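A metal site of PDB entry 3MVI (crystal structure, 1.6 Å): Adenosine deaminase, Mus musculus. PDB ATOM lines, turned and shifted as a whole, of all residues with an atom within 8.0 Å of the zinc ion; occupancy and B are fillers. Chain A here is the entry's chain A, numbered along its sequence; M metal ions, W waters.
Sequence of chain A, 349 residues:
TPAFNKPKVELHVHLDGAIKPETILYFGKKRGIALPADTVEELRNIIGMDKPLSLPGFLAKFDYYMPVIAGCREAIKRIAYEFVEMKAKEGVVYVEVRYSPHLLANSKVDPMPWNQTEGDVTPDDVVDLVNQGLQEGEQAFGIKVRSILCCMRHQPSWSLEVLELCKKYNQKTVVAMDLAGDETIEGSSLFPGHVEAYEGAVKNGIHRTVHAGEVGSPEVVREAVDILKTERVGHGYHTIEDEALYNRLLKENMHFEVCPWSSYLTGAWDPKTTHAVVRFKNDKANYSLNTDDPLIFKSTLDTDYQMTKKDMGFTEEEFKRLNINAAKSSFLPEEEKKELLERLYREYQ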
ATOM      1  N   HIS A  12      27.663  13.800   2.587  1.00  0.00           N
ATOM      2  CA  HIS A  12      26.599  13.419   3.527  1.00  0.00           C
ATOM      3  C   HIS A  12      25.207  13.624   2.887  1.00  0.00           C
ATOM      4  O   HIS A  12      24.625  14.711   2.978  1.00  0.00           O
ATOM      5  CB  HIS A  12      26.733  14.188   4.867  1.00  0.00           C
ATOM      6  CG  HIS A  12      25.849  13.656   5.956  1.00  0.00           C
ATOM      7  ND1 HIS A  12      26.329  13.266   7.190  1.00  0.00           N
ATOM      8  CD2 HIS A  12      24.502  13.410   5.980  1.00  0.00           C
ATOM      9  CE1 HIS A  12      25.331  12.805   7.922  1.00  0.00           C
ATOM     10  NE2 HIS A  12      24.207  12.891   7.213  1.00  0.00           N
ATOM     11  N   VAL A  13      24.685  12.562   2.289  1.00  0.00           N
ATOM     12  CA  VAL A  13      23.376  12.608   1.659  1.00  0.00           C
ATOM     13  C   VAL A  13      22.837  11.183   1.617  1.00  0.00           C
ATOM     14  O   VAL A  13      23.577  10.267   1.255  1.00  0.00           O
ATOM     15  CB  VAL A  13      23.410  13.254   0.206  1.00  0.00           C
ATOM     16  CG1 VAL A  13      24.453  12.602  -0.725  1.00  0.00           C
ATOM     17  CG2 VAL A  13      21.994  13.289  -0.454  1.00  0.00           C
ATOM     18  N   HIS A  14      21.575  11.014   2.046  1.00  0.00           N
ATOM     19  CA  HIS A  14      20.966   9.693   2.168  1.00  0.00           C
ATOM     20  C   HIS A  14      20.200   9.332   0.906  1.00  0.00           C
ATOM     21  O   HIS A  14      19.292  10.053   0.477  1.00  0.00           O
ATOM     22  CB  HIS A  14      20.021   9.672   3.390  1.00  0.00           C
ATOM     23  CG  HIS A  14      20.716   9.931   4.695  1.00  0.00           C
ATOM     24  ND1 HIS A  14      20.862   8.957   5.650  1.00  0.00           N
ATOM     25  CD2 HIS A  14      21.277  11.054   5.193  1.00  0.00           C
ATOM     26  CE1 HIS A  14      21.488   9.475   6.703  1.00  0.00           C
ATOM     27  NE2 HIS A  14      21.749  10.743   6.440  1.00  0.00           N
ATOM     28  N   LEU A  55      14.206  15.456  15.603  1.00  0.00           N
ATOM     29  CA  LEU A  55      14.793  14.315  14.888  1.00  0.00           C
ATOM     30  C   LEU A  55      13.783  13.157  14.759  1.00  0.00           C
ATOM     31  O   LEU A  55      13.575  12.649  13.659  1.00  0.00           O
ATOM     32  CB  LEU A  55      16.116  13.835  15.513  1.00  0.00           C
ATOM     33  CG  LEU A  55      16.955  12.922  14.605  1.00  0.00           C
ATOM     34  CD1 LEU A  55      17.331  13.643  13.290  1.00  0.00           C
ATOM     35  CD2 LEU A  55      18.199  12.400  15.313  1.00  0.00           C
ATOM     36  N   PHE A  58      11.076  14.144  12.230  1.00  0.00           N
ATOM     37  CA  PHE A  58      11.664  14.028  10.921  1.00  0.00           C
ATOM     38  C   PHE A  58      11.687  12.538  10.485  1.00  0.00           C
ATOM     39  O   PHE A  58      11.272  12.212   9.359  1.00  0.00           O
ATOM     40  CB  PHE A  58      13.085  14.636  10.945  1.00  0.00           C
ATOM     41  CG  PHE A  58      13.993  14.095   9.887  1.00  0.00           C
ATOM     42  CD1 PHE A  58      13.862  14.488   8.555  1.00  0.00           C
ATOM     43  CD2 PHE A  58      14.976  13.173  10.220  1.00  0.00           C
ATOM     44  CE1 PHE A  58      14.693  13.964   7.564  1.00  0.00           C
ATOM     45  CE2 PHE A  58      15.812  12.644   9.247  1.00  0.00           C
ATOM     46  CZ  PHE A  58      15.672  13.035   7.917  1.00  0.00           C
ATOM     47  N   ARG A  98      24.683   7.594   1.163  1.00  0.00           N
ATOM     48  CA  ARG A  98      24.520   6.562   2.180  1.00  0.00           C
ATOM     49  C   ARG A  98      23.112   6.063   2.385  1.00  0.00           C
ATOM     50  O   ARG A  98      22.151   6.786   2.184  1.00  0.00           O
ATOM     51  CB  ARG A  98      25.012   7.105   3.507  1.00  0.00           C
ATOM     52  CG  ARG A  98      24.184   8.245   4.048  1.00  0.00           C
ATOM     53  CD  ARG A  98      24.879   8.819   5.269  1.00  0.00           C
ATOM     54  NE  ARG A  98      26.123   9.506   4.943  1.00  0.00           N
ATOM     55  CZ  ARG A  98      26.955   9.988   5.869  1.00  0.00           C
ATOM     56  NH1 ARG A  98      26.680   9.815   7.170  1.00  0.00           N
ATOM     57  NH2 ARG A  98      28.068  10.615   5.485  1.00  0.00           N
ATOM     58  N   CYS A 150      24.819   2.267   6.241  1.00  0.00           N
ATOM     59  CA  CYS A 150      24.500   2.784   7.561  1.00  0.00           C
ATOM     60  C   CYS A 150      24.108   1.660   8.460  1.00  0.00           C
ATOM     61  O   CYS A 150      23.173   0.914   8.160  1.00  0.00           O
ATOM     62  CB  CYS A 150      23.317   3.746   7.513  1.00  0.00           C
ATOM     63  SG  CYS A 150      23.564   5.197   6.440  1.00  0.00           S
ATOM     64  N   ASP A 178      28.629   3.870   8.222  1.00  0.00           N
ATOM     65  CA  ASP A 178      28.075   5.000   8.990  1.00  0.00           C
ATOM     66  C   ASP A 178      27.195   4.430  10.100  1.00  0.00           C
ATOM     67  O   ASP A 178      26.835   3.239  10.098  1.00  0.00           O
ATOM     68  CB  ASP A 178      27.250   5.894   8.044  1.00  0.00           C
ATOM     69  CG  ASP A 178      26.555   7.089   8.759  1.00  0.00           C
ATOM     70  OD1 ASP A 178      27.125   7.736   9.679  1.00  0.00           O
ATOM     71  OD2 ASP A 178      25.405   7.406   8.344  1.00  0.00           O
ATOM     72  N   LEU A 179      26.870   5.295  11.068  1.00  0.00           N
ATOM     73  CA  LEU A 179      25.875   4.981  12.074  1.00  0.00           C
ATOM     74  C   LEU A 179      24.880   6.132  12.052  1.00  0.00           C
ATOM     75  O   LEU A 179      25.267   7.318  12.248  1.00  0.00           O
ATOM     76  CB  LEU A 179      26.539   4.864  13.433  1.00  0.00           C
ATOM     77  CG  LEU A 179      25.638   4.626  14.660  1.00  0.00           C
ATOM     78  CD1 LEU A 179      24.914   3.306  14.608  1.00  0.00           C
ATOM     79  CD2 LEU A 179      26.484   4.713  15.923  1.00  0.00           C
ATOM     80  N   ALA A 180      23.626   5.791  11.761  1.00  0.00           N
ATOM     81  CA  ALA A 180      22.567   6.786  11.519  1.00  0.00           C
ATOM     82  C   ALA A 180      21.369   6.426  12.382  1.00  0.00           C
ATOM     83  O   ALA A 180      21.414   5.486  13.170  1.00  0.00           O
ATOM     84  CB  ALA A 180      22.179   6.831  10.019  1.00  0.00           C
ATOM     85  N   GLY A 181      20.283   7.183  12.232  1.00  0.00           N
ATOM     86  CA  GLY A 181      19.081   6.867  12.958  1.00  0.00           C
ATOM     87  C   GLY A 181      18.900   7.809  14.136  1.00  0.00           C
ATOM     88  O   GLY A 181      19.399   8.943  14.130  1.00  0.00           O
ATOM     89  N   HIS A 211      27.075   9.708  12.546  1.00  0.00           N
ATOM     90  CA  HIS A 211      26.213  10.864  12.918  1.00  0.00           C
ATOM     91  C   HIS A 211      26.388  11.136  14.432  1.00  0.00           C
ATOM     92  O   HIS A 211      26.118  10.271  15.265  1.00  0.00           O
ATOM     93  CB  HIS A 211      24.725  10.549  12.703  1.00  0.00           C
ATOM     94  CG  HIS A 211      24.250  10.626  11.286  1.00  0.00           C
ATOM     95  ND1 HIS A 211      24.633   9.724  10.303  1.00  0.00           N
ATOM     96  CD2 HIS A 211      23.342  11.447  10.714  1.00  0.00           C
ATOM     97  CE1 HIS A 211      24.006  10.023   9.166  1.00  0.00           C
ATOM     98  NE2 HIS A 211      23.202  11.054   9.394  1.00  0.00           N
ATOM     99  N   GLU A 214      24.372  15.985  16.275  1.00  0.00           N
ATOM    100  CA  GLU A 214      23.296  16.588  15.451  1.00  0.00           C
ATOM    101  C   GLU A 214      22.242  17.107  16.422  1.00  0.00           C
ATOM    102  O   GLU A 214      21.988  18.316  16.465  1.00  0.00           O
ATOM    103  CB  GLU A 214      22.690  15.553  14.487  1.00  0.00           C
ATOM    104  CG  GLU A 214      21.562  16.112  13.600  1.00  0.00           C
ATOM    105  CD  GLU A 214      20.952  15.041  12.681  1.00  0.00           C
ATOM    106  OE1 GLU A 214      21.266  13.837  12.859  1.00  0.00           O
ATOM    107  OE2 GLU A 214      20.159  15.401  11.751  1.00  0.00           O
ATOM    108  N   GLY A 234      29.351  13.142  11.210  1.00  0.00           N
ATOM    109  CA  GLY A 234      28.094  13.656  10.652  1.00  0.00           C
ATOM    110  C   GLY A 234      27.505  14.748  11.515  1.00  0.00           C
ATOM    111  O   GLY A 234      27.098  14.468  12.638  1.00  0.00           O
ATOM    112  N   HIS A 235      27.436  15.965  10.980  1.00  0.00           N
ATOM    113  CA  HIS A 235      26.926  17.155  11.722  1.00  0.00           C
ATOM    114  C   HIS A 235      27.924  17.706  12.732  1.00  0.00           C
ATOM    115  O   HIS A 235      28.675  18.614  12.419  1.00  0.00           O
ATOM    116  CB  HIS A 235      25.565  16.883  12.382  1.00  0.00           C
ATOM    117  CG  HIS A 235      24.536  16.380  11.436  1.00  0.00           C
ATOM    118  ND1 HIS A 235      23.885  17.187  10.529  1.00  0.00           N
ATOM    119  CD2 HIS A 235      24.061  15.125  11.232  1.00  0.00           C
ATOM    120  CE1 HIS A 235      23.040  16.460   9.827  1.00  0.00           C
ATOM    121  NE2 HIS A 235      23.108  15.213  10.257  1.00  0.00           N
ATOM    122  N   GLU A 257      30.764  16.820   8.632  1.00  0.00           N
ATOM    123  CA  GLU A 257      29.874  16.817   7.478  1.00  0.00           C
ATOM    124  C   GLU A 257      28.671  17.690   7.826  1.00  0.00           C
ATOM    125  O   GLU A 257      27.730  17.243   8.483  1.00  0.00           O
ATOM    126  CB  GLU A 257      29.426  15.385   7.177  1.00  0.00           C
ATOM    127  CG  GLU A 257      30.579  14.384   7.062  1.00  0.00           C
ATOM    128  CD  GLU A 257      30.130  12.950   7.101  1.00  0.00           C
ATOM    129  OE1 GLU A 257      28.961  12.680   7.437  1.00  0.00           O
ATOM    130  OE2 GLU A 257      30.968  12.085   6.772  1.00  0.00           O
ATOM    131  N   CYS A 259      25.328  20.071   7.417  1.00  0.00           N
ATOM    132  CA  CYS A 259      24.080  20.024   6.649  1.00  0.00           C
ATOM    133  C   CYS A 259      23.174  21.173   7.116  1.00  0.00           C
ATOM    134  O   CYS A 259      22.284  20.972   7.935  1.00  0.00           O
ATOM    135  CB  CYS A 259      23.384  18.685   6.841  1.00  0.00           C
ATOM    136  SG  CYS A 259      24.395  17.228   6.530  1.00  0.00           S
ATOM    137  N   SER A 262      19.178  21.058   6.570  1.00  0.00           N
ATOM    138  CA  SER A 262      18.750  19.940   7.395  1.00  0.00           C
ATOM    139  C   SER A 262      18.679  20.336   8.876  1.00  0.00           C
ATOM    140  O   SER A 262      17.681  20.070   9.533  1.00  0.00           O
ATOM    141  CB  SER A 262      19.755  18.788   7.297  1.00  0.00           C
ATOM    142  OG  SER A 262      19.413  17.744   8.175  1.00  0.00           O
ATOM    143  N   ASN A 290      26.451  19.921   2.721  1.00  0.00           N
ATOM    144  CA  ASN A 290      25.747  18.685   2.324  1.00  0.00           C
ATOM    145  C   ASN A 290      24.242  18.846   2.446  1.00  0.00           C
ATOM    146  O   ASN A 290      23.769  19.564   3.316  1.00  0.00           O
ATOM    147  CB  ASN A 290      26.144  17.539   3.266  1.00  0.00           C
ATOM    148  CG  ASN A 290      27.638  17.325   3.302  1.00  0.00           C
ATOM    149  OD1 ASN A 290      28.338  17.854   4.200  1.00  0.00           O
ATOM    150  ND2 ASN A 290      28.144  16.614   2.330  1.00  0.00           N
ATOM    151  N   THR A 291      23.482  18.145   1.613  1.00  0.00           N
ATOM    152  CA  THR A 291      22.005  18.270   1.665  1.00  0.00           C
ATOM    153  C   THR A 291      21.314  17.388   2.695  1.00  0.00           C
ATOM    154  O   THR A 291      20.225  17.737   3.180  1.00  0.00           O
ATOM    155  CB  THR A 291      21.337  17.956   0.317  1.00  0.00           C
ATOM    156  OG1 THR A 291      21.736  16.643  -0.111  1.00  0.00           O
ATOM    157  CG2 THR A 291      21.710  18.999  -0.739  1.00  0.00           C
ATOM    158  N   ASP A 292      21.900  16.215   2.973  1.00  0.00           N
ATOM    159  CA  ASP A 292      21.347  15.264   3.971  1.00  0.00           C
ATOM    160  C   ASP A 292      20.118  14.467   3.421  1.00  0.00           C
ATOM    161  O   ASP A 292      20.257  13.297   3.023  1.00  0.00           O
ATOM    162  CB  ASP A 292      21.071  15.962   5.320  1.00  0.00           C
ATOM    163  CG  ASP A 292      21.043  14.995   6.480  1.00  0.00           C
ATOM    164  OD1 ASP A 292      21.454  13.837   6.274  1.00  0.00           O
ATOM    165  OD2 ASP A 292      20.588  15.387   7.576  1.00  0.00           O
ATOM    166  N   ASP A 293      18.934  15.093   3.419  1.00  0.00           N
ATOM    167  CA  ASP A 293      17.728  14.439   2.902  1.00  0.00           C
ATOM    168  C   ASP A 293      16.919  15.406   2.036  1.00  0.00           C
ATOM    169  O   ASP A 293      15.842  15.865   2.453  1.00  0.00           O
ATOM    170  CB  ASP A 293      16.854  13.897   4.028  1.00  0.00           C
ATOM    171  CG  ASP A 293      17.609  12.976   4.952  1.00  0.00           C
ATOM    172  OD1 ASP A 293      17.532  11.743   4.720  1.00  0.00           O
ATOM    173  OD2 ASP A 293      18.299  13.503   5.852  1.00  0.00           O
ATOM    174  N   PHE A 297      13.576  17.650   2.880  1.00  0.00           N
ATOM    175  CA  PHE A 297      13.829  19.064   3.118  1.00  0.00           C
ATOM    176  C   PHE A 297      13.461  19.970   1.944  1.00  0.00           C
ATOM    177  O   PHE A 297      13.628  21.188   2.012  1.00  0.00           O
ATOM    178  CB  PHE A 297      15.286  19.275   3.537  1.00  0.00           C
ATOM    179  CG  PHE A 297      15.682  18.449   4.747  1.00  0.00           C
ATOM    180  CD1 PHE A 297      14.792  18.313   5.829  1.00  0.00           C
ATOM    181  CD2 PHE A 297      16.905  17.791   4.805  1.00  0.00           C
ATOM    182  CE1 PHE A 297      15.122  17.557   6.947  1.00  0.00           C
ATOM    183  CE2 PHE A 297      17.239  17.016   5.917  1.00  0.00           C
ATOM    184  CZ  PHE A 297      16.362  16.899   6.979  1.00  0.00           C
HETATM  185 ZN    ZN M   1      22.360  12.201   7.785  1.00  0.00          ZN
HETATM  186  O   HOH W   1      21.344  13.357   9.156  1.00  0.00           O
HETATM  187  O   HOH W   2      19.163  12.477   7.861  1.00  0.00           O
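Merely in contact with the zinc ion: His 235 (3.97 Å). Within 4 Å of the zinc ion: His 12, His 14, His 211, His 235 and Asp 292.
The zinc ion is bound by NE2 of His 12, at 2.1 Å. Water W1 is bound to the zinc ion. The zinc ion is bound by NE2 of His 14. A ring nitrogen (NE2) of His 211 binds the zinc ion (2.1 Å). The zinc ion is bound by the side-chain carboxylate (OD1) of Asp 292, 2.4 Å away. The zinc ion has five donor atoms within binding distance.
Water W1 bridges the side-chain carboxylate of Asp 292 (2.7 Å) and a ring nitrogen (NE2) of His 235 (2.8 Å). Water W2 lies within hydrogen-bond range of the side-chain carboxylate (OD2) of Asp 293 and the side-chain carboxylate (OD2) of Asp 292.
ND1 of His 12 lies close to NH1 of Arg 98 (3.5 Å). ND1 of His 12 lies within hydrogen-bond range of OE1 of Glu 257 (2.7 Å). ND2 of Asn 290 sits close to N of His 12 (2.9 Å). A ring nitrogen (ND1) of His 211 sits close to the side-chain carboxylate (OD2) of Asp 178, at 3.1 Å. O of Leu 179 is in hydrogen-bond range of N of His 211, at 3.0 Å. The side-chain hydroxyl of Ser 262 is in hydrogen-bond range of the side-chain carboxylate of Asp 292. A ring nitrogen (NE2) of His 235 sits close to the side-chain carboxylate (OE2) of Glu 214 (3.3 Å). The backbone carbonyl oxygen (O) of Glu 257 lies within hydrogen-bond range of the backbone NH (N) of His 235.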
